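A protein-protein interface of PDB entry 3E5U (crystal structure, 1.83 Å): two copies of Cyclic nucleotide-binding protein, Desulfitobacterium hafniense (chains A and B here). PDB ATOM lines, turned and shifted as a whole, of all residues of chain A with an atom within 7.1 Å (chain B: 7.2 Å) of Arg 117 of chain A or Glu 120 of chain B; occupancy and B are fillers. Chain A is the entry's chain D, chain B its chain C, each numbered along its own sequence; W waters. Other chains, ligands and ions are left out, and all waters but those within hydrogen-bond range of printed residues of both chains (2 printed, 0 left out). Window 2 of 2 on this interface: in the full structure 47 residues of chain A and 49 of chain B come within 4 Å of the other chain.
Water W2 bridges NH2 of Arg 113 of chain A (2.9 Å) and OD1 of Asp 121 of chain B (3.4 Å).
Water W1 lies within hydrogen-bond range of O of Arg 113 of chain A (3.3 Å) and OE1 of Glu 120 of chain B (3.4 Å).
OE2 of Glu 109 of chain A is in salt-bridge range of NH2 of Arg 113 of chain A (3.4 Å).
The backbone NH of Asp 121 of chain B lies close to the side-chain carboxylate of Asp 119 of chain B, at 3.4 Å.
Of the printed residues of chain B, Phe 116 of chain A touches Ile 123 and Phe 124.
Arg 117 of chain A touches just one residue of chain B: Glu 120 (3.0 Å).
Printed residues of chain B within 4 Å of Glu 120 of chain A: Arg 117.
Glu 120 of chain B touches two residues of chain A.
Printed residues of chain A within 4 Å of Ile 123 of chain B: Phe 116 (3.8 Å) and Ile 123 (3.7 Å).
The nearest printed residue of chain A that does not touch Arg 117 of chain B is Ile 123 of chain A (6.8 Å).
Phe 116 of chain A touches Ile 123 of chain B, and with the chains exchanged Ile 123 of chain A touches Phe 116 of chain B.
Arg 117 of chain A touches Glu 120 of chain B, and with the chains exchanged Glu 120 of chain A touches Arg 117 of chain B.
Ile 123 of chain B touches its own counterpart, Ile 123 of chain A.
7 positions are printed for both chains.
OE1 of Glu 120 of chain B lies within salt-bridge range of NH2 of Arg 117 of chain A, 3.0 Å away.
The side-chain carboxylate (OD1) of Asp 121 of chain B is in salt-bridge range of the guanidinium group (NH1) of Arg 113 of chain A (2.9 Å).
The guanidinium group of Arg 113 of chain A is in salt-bridge range of the side-chain carboxylate of Glu 120 of chain B, 2.7 Å away.
The guanidinium group of Arg 117 of chain B lies within salt-bridge range of the side-chain carboxylate of Glu 120 of chain A (2.8 Å).
CG of Glu 109 of chain A touches CE2 of Phe 124 of chain B, 3.8 Å away.
CZ of Phe 124 of chain B touches CG of Arg 113 of chain A, 3.6 Å away.
Phe 116 of chain A touches Ile 123 of chain B.
CZ of Phe 124 of chain B touches CE2 of Phe 116 of chain A (3.6 Å).
Phe 116 of chain B touches Ile 123 of chain A (CE2 to CG2, 3.8 Å).
Ile 123 of chain A touches Ile 123 of chain B.
Hydrophobic or aromatic side chains of chain B within 4 Å of the printed part of chain A: Phe 116, Ile 123 and Phe 124.
Along chain B the printed residues that touch a printed residue of chain A span positions 116 to 124.
Hydrophobic or aromatic side chains of chain A that line the printed part of chain B: Phe 116 and Ile 123.
Among the printed residues, 10 pairs touch across the chains.
Among the printed residues, Asp or Glu carboxylates within 4 Å of a Lys or Arg side-chain nitrogen of the other chain: Arg 113 of chain A with Glu 120 of chain B, Arg 113 of chain A with Asp 121 of chain B, Arg 117 of chain A with Glu 120 of chain B and Glu 120 of chain A with Arg 117 of chain B.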
ATOM      1  N   GLU A 109      -8.408  -6.732  -9.578  1.00  0.00           N
ATOM      2  CA  GLU A 109      -7.981  -7.243  -8.265  1.00  0.00           C
ATOM      3  C   GLU A 109      -8.996  -8.162  -7.609  1.00  0.00           C
ATOM      4  O   GLU A 109      -8.688  -9.265  -7.149  1.00  0.00           O
ATOM      5  CB  GLU A 109      -7.621  -6.094  -7.342  1.00  0.00           C
ATOM      6  CG  GLU A 109      -6.965  -6.616  -6.088  1.00  0.00           C
ATOM      7  CD  GLU A 109      -6.867  -5.544  -5.012  1.00  0.00           C
ATOM      8  OE1 GLU A 109      -5.817  -4.901  -4.935  1.00  0.00           O
ATOM      9  OE2 GLU A 109      -7.799  -5.398  -4.203  1.00  0.00           O
ATOM     10  N   LYS A 110     -10.255  -7.771  -7.665  1.00  0.00           N
ATOM     11  CA  LYS A 110     -11.348  -8.577  -7.113  1.00  0.00           C
ATOM     12  C   LYS A 110     -11.443  -9.928  -7.861  1.00  0.00           C
ATOM     13  O   LYS A 110     -11.608 -10.980  -7.268  1.00  0.00           O
ATOM     14  CB  LYS A 110     -12.675  -7.764  -7.261  1.00  0.00           C
ATOM     15  CG  LYS A 110     -13.928  -8.414  -6.584  1.00  0.00           C
ATOM     16  CD  LYS A 110     -15.180  -7.501  -6.746  1.00  0.00           C
ATOM     17  CE  LYS A 110     -16.530  -8.252  -6.741  1.00  0.00           C
ATOM     18  NZ  LYS A 110     -16.835  -8.989  -5.456  1.00  0.00           N
ATOM     19  N   SER A 111     -11.331  -9.888  -9.189  1.00  0.00           N
ATOM     20  CA  SER A 111     -11.344 -11.112  -9.993  1.00  0.00           C
ATOM     21  C   SER A 111     -10.225 -12.045  -9.570  1.00  0.00           C
ATOM     22  O   SER A 111     -10.417 -13.288  -9.514  1.00  0.00           O
ATOM     23  CB  SER A 111     -11.183 -10.824 -11.511  1.00  0.00           C
ATOM     24  OG  SER A 111     -12.330 -10.079 -11.980  1.00  0.00           O
ATOM     25  N   LEU A 112      -9.028 -11.478  -9.397  1.00  0.00           N
ATOM     26  CA  LEU A 112      -7.865 -12.287  -9.026  1.00  0.00           C
ATOM     27  C   LEU A 112      -8.032 -12.937  -7.657  1.00  0.00           C
ATOM     28  O   LEU A 112      -7.612 -14.072  -7.421  1.00  0.00           O
ATOM     29  CB  LEU A 112      -6.573 -11.443  -9.084  1.00  0.00           C
ATOM     30  CG  LEU A 112      -6.027 -11.124 -10.505  1.00  0.00           C
ATOM     31  CD1 LEU A 112      -4.829 -10.115 -10.449  1.00  0.00           C
ATOM     32  CD2 LEU A 112      -5.646 -12.351 -11.338  1.00  0.00           C
ATOM     33  N   ARG A 113      -8.611 -12.199  -6.728  1.00  0.00           N
ATOM     34  CA  ARG A 113      -8.934 -12.752  -5.436  1.00  0.00           C
ATOM     35  C   ARG A 113      -9.802 -14.022  -5.597  1.00  0.00           C
ATOM     36  O   ARG A 113      -9.525 -15.012  -4.961  1.00  0.00           O
ATOM     37  CB  ARG A 113      -9.678 -11.748  -4.567  1.00  0.00           C
ATOM     38  CG  ARG A 113      -8.835 -10.653  -4.033  1.00  0.00           C
ATOM     39  CD  ARG A 113      -9.582  -9.689  -3.086  1.00  0.00           C
ATOM     40  NE  ARG A 113      -8.778  -8.531  -2.762  1.00  0.00           N
ATOM     41  CZ  ARG A 113      -7.854  -8.507  -1.802  1.00  0.00           C
ATOM     42  NH1 ARG A 113      -7.595  -9.578  -1.009  1.00  0.00           N
ATOM     43  NH2 ARG A 113      -7.153  -7.427  -1.613  1.00  0.00           N
ATOM     44  N   THR A 114     -10.815 -14.005  -6.458  1.00  0.00           N
ATOM     45  CA  THR A 114     -11.575 -15.224  -6.779  1.00  0.00           C
ATOM     46  C   THR A 114     -10.742 -16.350  -7.408  1.00  0.00           C
ATOM     47  O   THR A 114     -10.893 -17.518  -6.991  1.00  0.00           O
ATOM     48  CB  THR A 114     -12.788 -14.903  -7.713  1.00  0.00           C
ATOM     49  OG1 THR A 114     -13.561 -13.892  -7.071  1.00  0.00           O
ATOM     50  CG2 THR A 114     -13.677 -16.142  -7.900  1.00  0.00           C
ATOM     51  N   VAL A 115      -9.851 -15.996  -8.344  1.00  0.00           N
ATOM     52  CA  VAL A 115      -8.898 -16.966  -8.898  1.00  0.00           C
ATOM     53  C   VAL A 115      -8.038 -17.655  -7.780  1.00  0.00           C
ATOM     54  O   VAL A 115      -7.938 -18.875  -7.761  1.00  0.00           O
ATOM     55  CB  VAL A 115      -8.029 -16.389 -10.028  1.00  0.00           C
ATOM     56  CG1 VAL A 115      -6.904 -17.391 -10.418  1.00  0.00           C
ATOM     57  CG2 VAL A 115      -8.862 -15.855 -11.255  1.00  0.00           C
ATOM     58  N   PHE A 116      -7.451 -16.883  -6.855  1.00  0.00           N
ATOM     59  CA  PHE A 116      -6.478 -17.431  -5.905  1.00  0.00           C
ATOM     60  C   PHE A 116      -7.204 -18.232  -4.850  1.00  0.00           C
ATOM     61  O   PHE A 116      -6.666 -19.244  -4.281  1.00  0.00           O
ATOM     62  CB  PHE A 116      -5.630 -16.299  -5.296  1.00  0.00           C
ATOM     63  CG  PHE A 116      -4.893 -15.456  -6.306  1.00  0.00           C
ATOM     64  CD1 PHE A 116      -4.391 -15.981  -7.533  1.00  0.00           C
ATOM     65  CD2 PHE A 116      -4.718 -14.098  -6.064  1.00  0.00           C
ATOM     66  CE1 PHE A 116      -3.703 -15.212  -8.448  1.00  0.00           C
ATOM     67  CE2 PHE A 116      -4.030 -13.330  -6.991  1.00  0.00           C
ATOM     68  CZ  PHE A 116      -3.513 -13.900  -8.210  1.00  0.00           C
ATOM     69  N   ARG A 117      -8.443 -17.815  -4.561  1.00  0.00           N
ATOM     70  CA  ARG A 117      -9.298 -18.567  -3.615  1.00  0.00           C
ATOM     71  C   ARG A 117      -9.665 -19.925  -4.202  1.00  0.00           C
ATOM     72  O   ARG A 117      -9.926 -20.883  -3.477  1.00  0.00           O
ATOM     73  CB  ARG A 117     -10.565 -17.781  -3.232  1.00  0.00           C
ATOM     74  CG  ARG A 117     -10.330 -16.567  -2.346  1.00  0.00           C
ATOM     75  CD  ARG A 117     -11.518 -15.654  -2.410  1.00  0.00           C
ATOM     76  NE  ARG A 117     -11.254 -14.354  -1.802  1.00  0.00           N
ATOM     77  CZ  ARG A 117     -12.070 -13.304  -1.887  1.00  0.00           C
ATOM     78  NH1 ARG A 117     -13.224 -13.386  -2.571  1.00  0.00           N
ATOM     79  NH2 ARG A 117     -11.728 -12.166  -1.297  1.00  0.00           N
ATOM     80  N   THR A 118      -9.743 -20.003  -5.510  1.00  0.00           N
ATOM     81  CA  THR A 118      -9.982 -21.277  -6.195  1.00  0.00           C
ATOM     82  C   THR A 118      -8.716 -22.099  -6.373  1.00  0.00           C
ATOM     83  O   THR A 118      -8.774 -23.333  -6.351  1.00  0.00           O
ATOM     84  CB  THR A 118     -10.625 -21.007  -7.618  1.00  0.00           C
ATOM     85  OG1 THR A 118     -11.684 -20.022  -7.464  1.00  0.00           O
ATOM     86  CG2 THR A 118     -11.208 -22.264  -8.249  1.00  0.00           C
ATOM     87  N   ASP A 119      -7.578 -21.422  -6.628  1.00  0.00           N
ATOM     88  CA  ASP A 119      -6.359 -22.122  -7.027  1.00  0.00           C
ATOM     89  C   ASP A 119      -5.118 -21.378  -6.583  1.00  0.00           C
ATOM     90  O   ASP A 119      -4.600 -20.462  -7.273  1.00  0.00           O
ATOM     91  CB  ASP A 119      -6.383 -22.343  -8.550  1.00  0.00           C
ATOM     92  CG  ASP A 119      -5.502 -23.492  -8.992  1.00  0.00           C
ATOM     93  OD1 ASP A 119      -5.748 -24.663  -8.667  1.00  0.00           O
ATOM     94  OD2 ASP A 119      -4.601 -23.215  -9.746  1.00  0.00           O
ATOM     95  N   GLU A 120      -4.684 -21.743  -5.359  1.00  0.00           N
ATOM     96  CA  GLU A 120      -3.484 -21.163  -4.712  1.00  0.00           C
ATOM     97  C   GLU A 120      -2.321 -21.152  -5.648  1.00  0.00           C
ATOM     98  O   GLU A 120      -1.509 -20.216  -5.650  1.00  0.00           O
ATOM     99  CB  GLU A 120      -3.140 -21.985  -3.469  1.00  0.00           C
ATOM    100  CG  GLU A 120      -1.977 -21.524  -2.640  1.00  0.00           C
ATOM    101  CD  GLU A 120      -1.880 -22.370  -1.362  1.00  0.00           C
ATOM    102  OE1 GLU A 120      -1.121 -23.355  -1.378  1.00  0.00           O
ATOM    103  OE2 GLU A 120      -2.653 -22.125  -0.437  1.00  0.00           O
ATOM    104  N   ILE A 123      -1.097 -17.951  -7.781  1.00  0.00           N
ATOM    105  CA  ILE A 123      -0.298 -16.927  -7.149  1.00  0.00           C
ATOM    106  C   ILE A 123       1.157 -17.021  -7.586  1.00  0.00           C
ATOM    107  O   ILE A 123       1.744 -16.036  -7.985  1.00  0.00           O
ATOM    108  CB  ILE A 123      -0.329 -17.074  -5.631  1.00  0.00           C
ATOM    109  CG1 ILE A 123      -1.763 -16.849  -5.065  1.00  0.00           C
ATOM    110  CG2 ILE A 123       0.619 -16.030  -5.000  1.00  0.00           C
ATOM    111  CD1 ILE A 123      -2.023 -17.496  -3.705  1.00  0.00           C
ATOM    112  N   TYR B  28       4.175 -11.629  10.056  1.00  0.00           N
ATOM    113  CA  TYR B  28       4.245 -13.029   9.681  1.00  0.00           C
ATOM    114  C   TYR B  28       5.679 -13.645   9.768  1.00  0.00           C
ATOM    115  O   TYR B  28       5.921 -14.766   9.325  1.00  0.00           O
ATOM    116  CB  TYR B  28       3.588 -13.213   8.307  1.00  0.00           C
ATOM    117  CG  TYR B  28       2.197 -12.667   8.259  1.00  0.00           C
ATOM    118  CD1 TYR B  28       1.912 -11.500   7.581  1.00  0.00           C
ATOM    119  CD2 TYR B  28       1.195 -13.280   8.957  1.00  0.00           C
ATOM    120  CE1 TYR B  28       0.644 -10.990   7.542  1.00  0.00           C
ATOM    121  CE2 TYR B  28      -0.089 -12.761   8.977  1.00  0.00           C
ATOM    122  CZ  TYR B  28      -0.357 -11.616   8.265  1.00  0.00           C
ATOM    123  OH  TYR B  28      -1.609 -11.132   8.317  1.00  0.00           O
ATOM    124  N   VAL B 115       1.523 -18.129   4.757  1.00  0.00           N
ATOM    125  CA  VAL B 115       1.151 -16.657   4.858  1.00  0.00           C
ATOM    126  C   VAL B 115      -0.150 -16.350   4.113  1.00  0.00           C
ATOM    127  O   VAL B 115      -1.056 -15.702   4.671  1.00  0.00           O
ATOM    128  CB  VAL B 115       2.252 -15.682   4.371  1.00  0.00           C
ATOM    129  CG1 VAL B 115       1.725 -14.166   4.322  1.00  0.00           C
ATOM    130  CG2 VAL B 115       3.533 -15.804   5.214  1.00  0.00           C
ATOM    131  N   PHE B 116      -0.263 -16.837   2.865  1.00  0.00           N
ATOM    132  CA  PHE B 116      -1.418 -16.495   2.052  1.00  0.00           C
ATOM    133  C   PHE B 116      -2.702 -17.189   2.465  1.00  0.00           C
ATOM    134  O   PHE B 116      -3.792 -16.645   2.314  1.00  0.00           O
ATOM    135  CB  PHE B 116      -1.122 -16.746   0.560  1.00  0.00           C
ATOM    136  CG  PHE B 116       0.108 -16.044   0.038  1.00  0.00           C
ATOM    137  CD1 PHE B 116       0.523 -14.782   0.517  1.00  0.00           C
ATOM    138  CD2 PHE B 116       0.852 -16.666  -0.946  1.00  0.00           C
ATOM    139  CE1 PHE B 116       1.687 -14.130   0.029  1.00  0.00           C
ATOM    140  CE2 PHE B 116       2.009 -16.068  -1.430  1.00  0.00           C
ATOM    141  CZ  PHE B 116       2.400 -14.753  -1.006  1.00  0.00           C
ATOM    142  N   ARG B 117      -2.571 -18.374   3.034  1.00  0.00           N
ATOM    143  CA  ARG B 117      -3.708 -19.092   3.626  1.00  0.00           C
ATOM    144  C   ARG B 117      -4.293 -18.351   4.852  1.00  0.00           C
ATOM    145  O   ARG B 117      -5.459 -18.512   5.246  1.00  0.00           O
ATOM    146  CB  ARG B 117      -3.323 -20.539   3.957  1.00  0.00           C
ATOM    147  CG  ARG B 117      -3.115 -21.458   2.739  1.00  0.00           C
ATOM    148  CD  ARG B 117      -2.512 -22.789   3.214  1.00  0.00           C
ATOM    149  NE  ARG B 117      -2.070 -23.524   2.030  1.00  0.00           N
ATOM    150  CZ  ARG B 117      -1.404 -24.647   2.014  1.00  0.00           C
ATOM    151  NH1 ARG B 117      -1.135 -25.349   3.128  1.00  0.00           N
ATOM    152  NH2 ARG B 117      -1.061 -25.114   0.825  1.00  0.00           N
ATOM    153  N   THR B 118      -3.431 -17.600   5.506  1.00  0.00           N
ATOM    154  CA  THR B 118      -3.771 -16.781   6.670  1.00  0.00           C
ATOM    155  C   THR B 118      -4.337 -15.422   6.340  1.00  0.00           C
ATOM    156  O   THR B 118      -5.274 -14.937   7.008  1.00  0.00           O
ATOM    157  CB  THR B 118      -2.474 -16.598   7.549  1.00  0.00           C
ATOM    158  OG1 THR B 118      -1.943 -17.890   7.937  1.00  0.00           O
ATOM    159  CG2 THR B 118      -2.726 -15.775   8.753  1.00  0.00           C
ATOM    160  N   ASP B 119      -3.708 -14.755   5.360  1.00  0.00           N
ATOM    161  CA  ASP B 119      -4.005 -13.340   5.043  1.00  0.00           C
ATOM    162  C   ASP B 119      -3.772 -13.134   3.511  1.00  0.00           C
ATOM    163  O   ASP B 119      -2.668 -12.894   3.061  1.00  0.00           O
ATOM    164  CB  ASP B 119      -3.098 -12.388   5.880  1.00  0.00           C
ATOM    165  CG  ASP B 119      -3.445 -10.936   5.672  1.00  0.00           C
ATOM    166  OD1 ASP B 119      -4.504 -10.654   5.091  1.00  0.00           O
ATOM    167  OD2 ASP B 119      -2.713 -10.112   6.136  1.00  0.00           O
ATOM    168  N   GLU B 120      -4.850 -13.204   2.756  1.00  0.00           N
ATOM    169  CA  GLU B 120      -4.763 -13.075   1.325  1.00  0.00           C
ATOM    170  C   GLU B 120      -4.308 -11.741   0.860  1.00  0.00           C
ATOM    171  O   GLU B 120      -3.802 -11.633  -0.205  1.00  0.00           O
ATOM    172  CB  GLU B 120      -6.062 -13.502   0.658  1.00  0.00           C
ATOM    173  CG  GLU B 120      -7.197 -12.599   0.846  1.00  0.00           C
ATOM    174  CD  GLU B 120      -8.414 -12.927  -0.017  1.00  0.00           C
ATOM    175  OE1 GLU B 120      -8.832 -12.006  -0.735  1.00  0.00           O
ATOM    176  OE2 GLU B 120      -9.048 -13.977   0.178  1.00  0.00           O
ATOM    177  N   ASP B 121      -4.519 -10.680   1.648  1.00  0.00           N
ATOM    178  CA  ASP B 121      -3.998  -9.358   1.266  1.00  0.00           C
ATOM    179  C   ASP B 121      -2.504  -9.336   0.988  1.00  0.00           C
ATOM    180  O   ASP B 121      -1.981  -8.467   0.255  1.00  0.00           O
ATOM    181  CB  ASP B 121      -4.377  -8.325   2.350  1.00  0.00           C
ATOM    182  CG  ASP B 121      -5.813  -7.865   2.245  1.00  0.00           C
ATOM    183  OD1 ASP B 121      -6.480  -8.066   1.201  1.00  0.00           O
ATOM    184  OD2 ASP B 121      -6.242  -7.221   3.235  1.00  0.00           O
ATOM    185  N   MET B 122      -1.743 -10.254   1.581  1.00  0.00           N
ATOM    186  CA  MET B 122      -0.257 -10.194   1.391  1.00  0.00           C
ATOM    187  C   MET B 122       0.148 -10.547  -0.026  1.00  0.00           C
ATOM    188  O   MET B 122       1.205 -10.128  -0.481  1.00  0.00           O
ATOM    189  CB  MET B 122       0.455 -11.110   2.384  1.00  0.00           C
ATOM    190  CG  MET B 122       0.220 -10.719   3.855  1.00  0.00           C
ATOM    191  SD  MET B 122       0.747  -9.032   4.174  1.00  0.00           S
ATOM    192  CE  MET B 122      -0.563  -7.944   3.907  1.00  0.00           C
ATOM    193  N   ILE B 123      -0.662 -11.368  -0.678  1.00  0.00           N
ATOM    194  CA  ILE B 123      -0.503 -11.618  -2.099  1.00  0.00           C
ATOM    195  C   ILE B 123      -0.277 -10.311  -2.901  1.00  0.00           C
ATOM    196  O   ILE B 123       0.655 -10.174  -3.733  1.00  0.00           O
ATOM    197  CB  ILE B 123      -1.709 -12.409  -2.699  1.00  0.00           C
ATOM    198  CG1 ILE B 123      -1.932 -13.785  -2.014  1.00  0.00           C
ATOM    199  CG2 ILE B 123      -1.514 -12.691  -4.252  1.00  0.00           C
ATOM    200  CD1 ILE B 123      -3.326 -14.391  -2.239  1.00  0.00           C
ATOM    201  N   PHE B 124      -1.189  -9.375  -2.673  1.00  0.00           N
ATOM    202  CA  PHE B 124      -1.293  -8.195  -3.490  1.00  0.00           C
ATOM    203  C   PHE B 124      -0.242  -7.206  -3.133  1.00  0.00           C
ATOM    204  O   PHE B 124       0.221  -6.522  -4.002  1.00  0.00           O
ATOM    205  CB  PHE B 124      -2.715  -7.634  -3.472  1.00  0.00           C
ATOM    206  CG  PHE B 124      -3.717  -8.607  -3.998  1.00  0.00           C
ATOM    207  CD1 PHE B 124      -4.315  -9.559  -3.153  1.00  0.00           C
ATOM    208  CD2 PHE B 124      -3.937  -8.729  -5.369  1.00  0.00           C
ATOM    209  CE1 PHE B 124      -5.178 -10.557  -3.697  1.00  0.00           C
ATOM    210  CE2 PHE B 124      -4.812  -9.683  -5.875  1.00  0.00           C
ATOM    211  CZ  PHE B 124      -5.417 -10.602  -5.058  1.00  0.00           C
ATOM    212  N   GLU B 125       0.182  -7.145  -1.851  1.00  0.00           N
ATOM    213  CA  GLU B 125       1.349  -6.314  -1.543  1.00  0.00           C
ATOM    214  C   GLU B 125       2.632  -6.790  -2.232  1.00  0.00           C
ATOM    215  O   GLU B 125       3.407  -5.992  -2.668  1.00  0.00           O
ATOM    216  CB  GLU B 125       1.560  -6.204  -0.025  1.00  0.00           C
ATOM    217  CG  GLU B 125       0.328  -5.602   0.725  1.00  0.00           C
ATOM    218  CD  GLU B 125      -0.123  -4.286   0.120  1.00  0.00           C
ATOM    219  OE1 GLU B 125      -1.293  -4.170  -0.344  1.00  0.00           O
ATOM    220  OE2 GLU B 125       0.653  -3.315   0.226  1.00  0.00           O
HETATM  221  O   HOH W   1      -7.239 -14.235  -2.779  1.00  0.00           O
HETATM  222  O   HOH W   2      -5.530  -5.264  -0.473  1.00  0.00           O
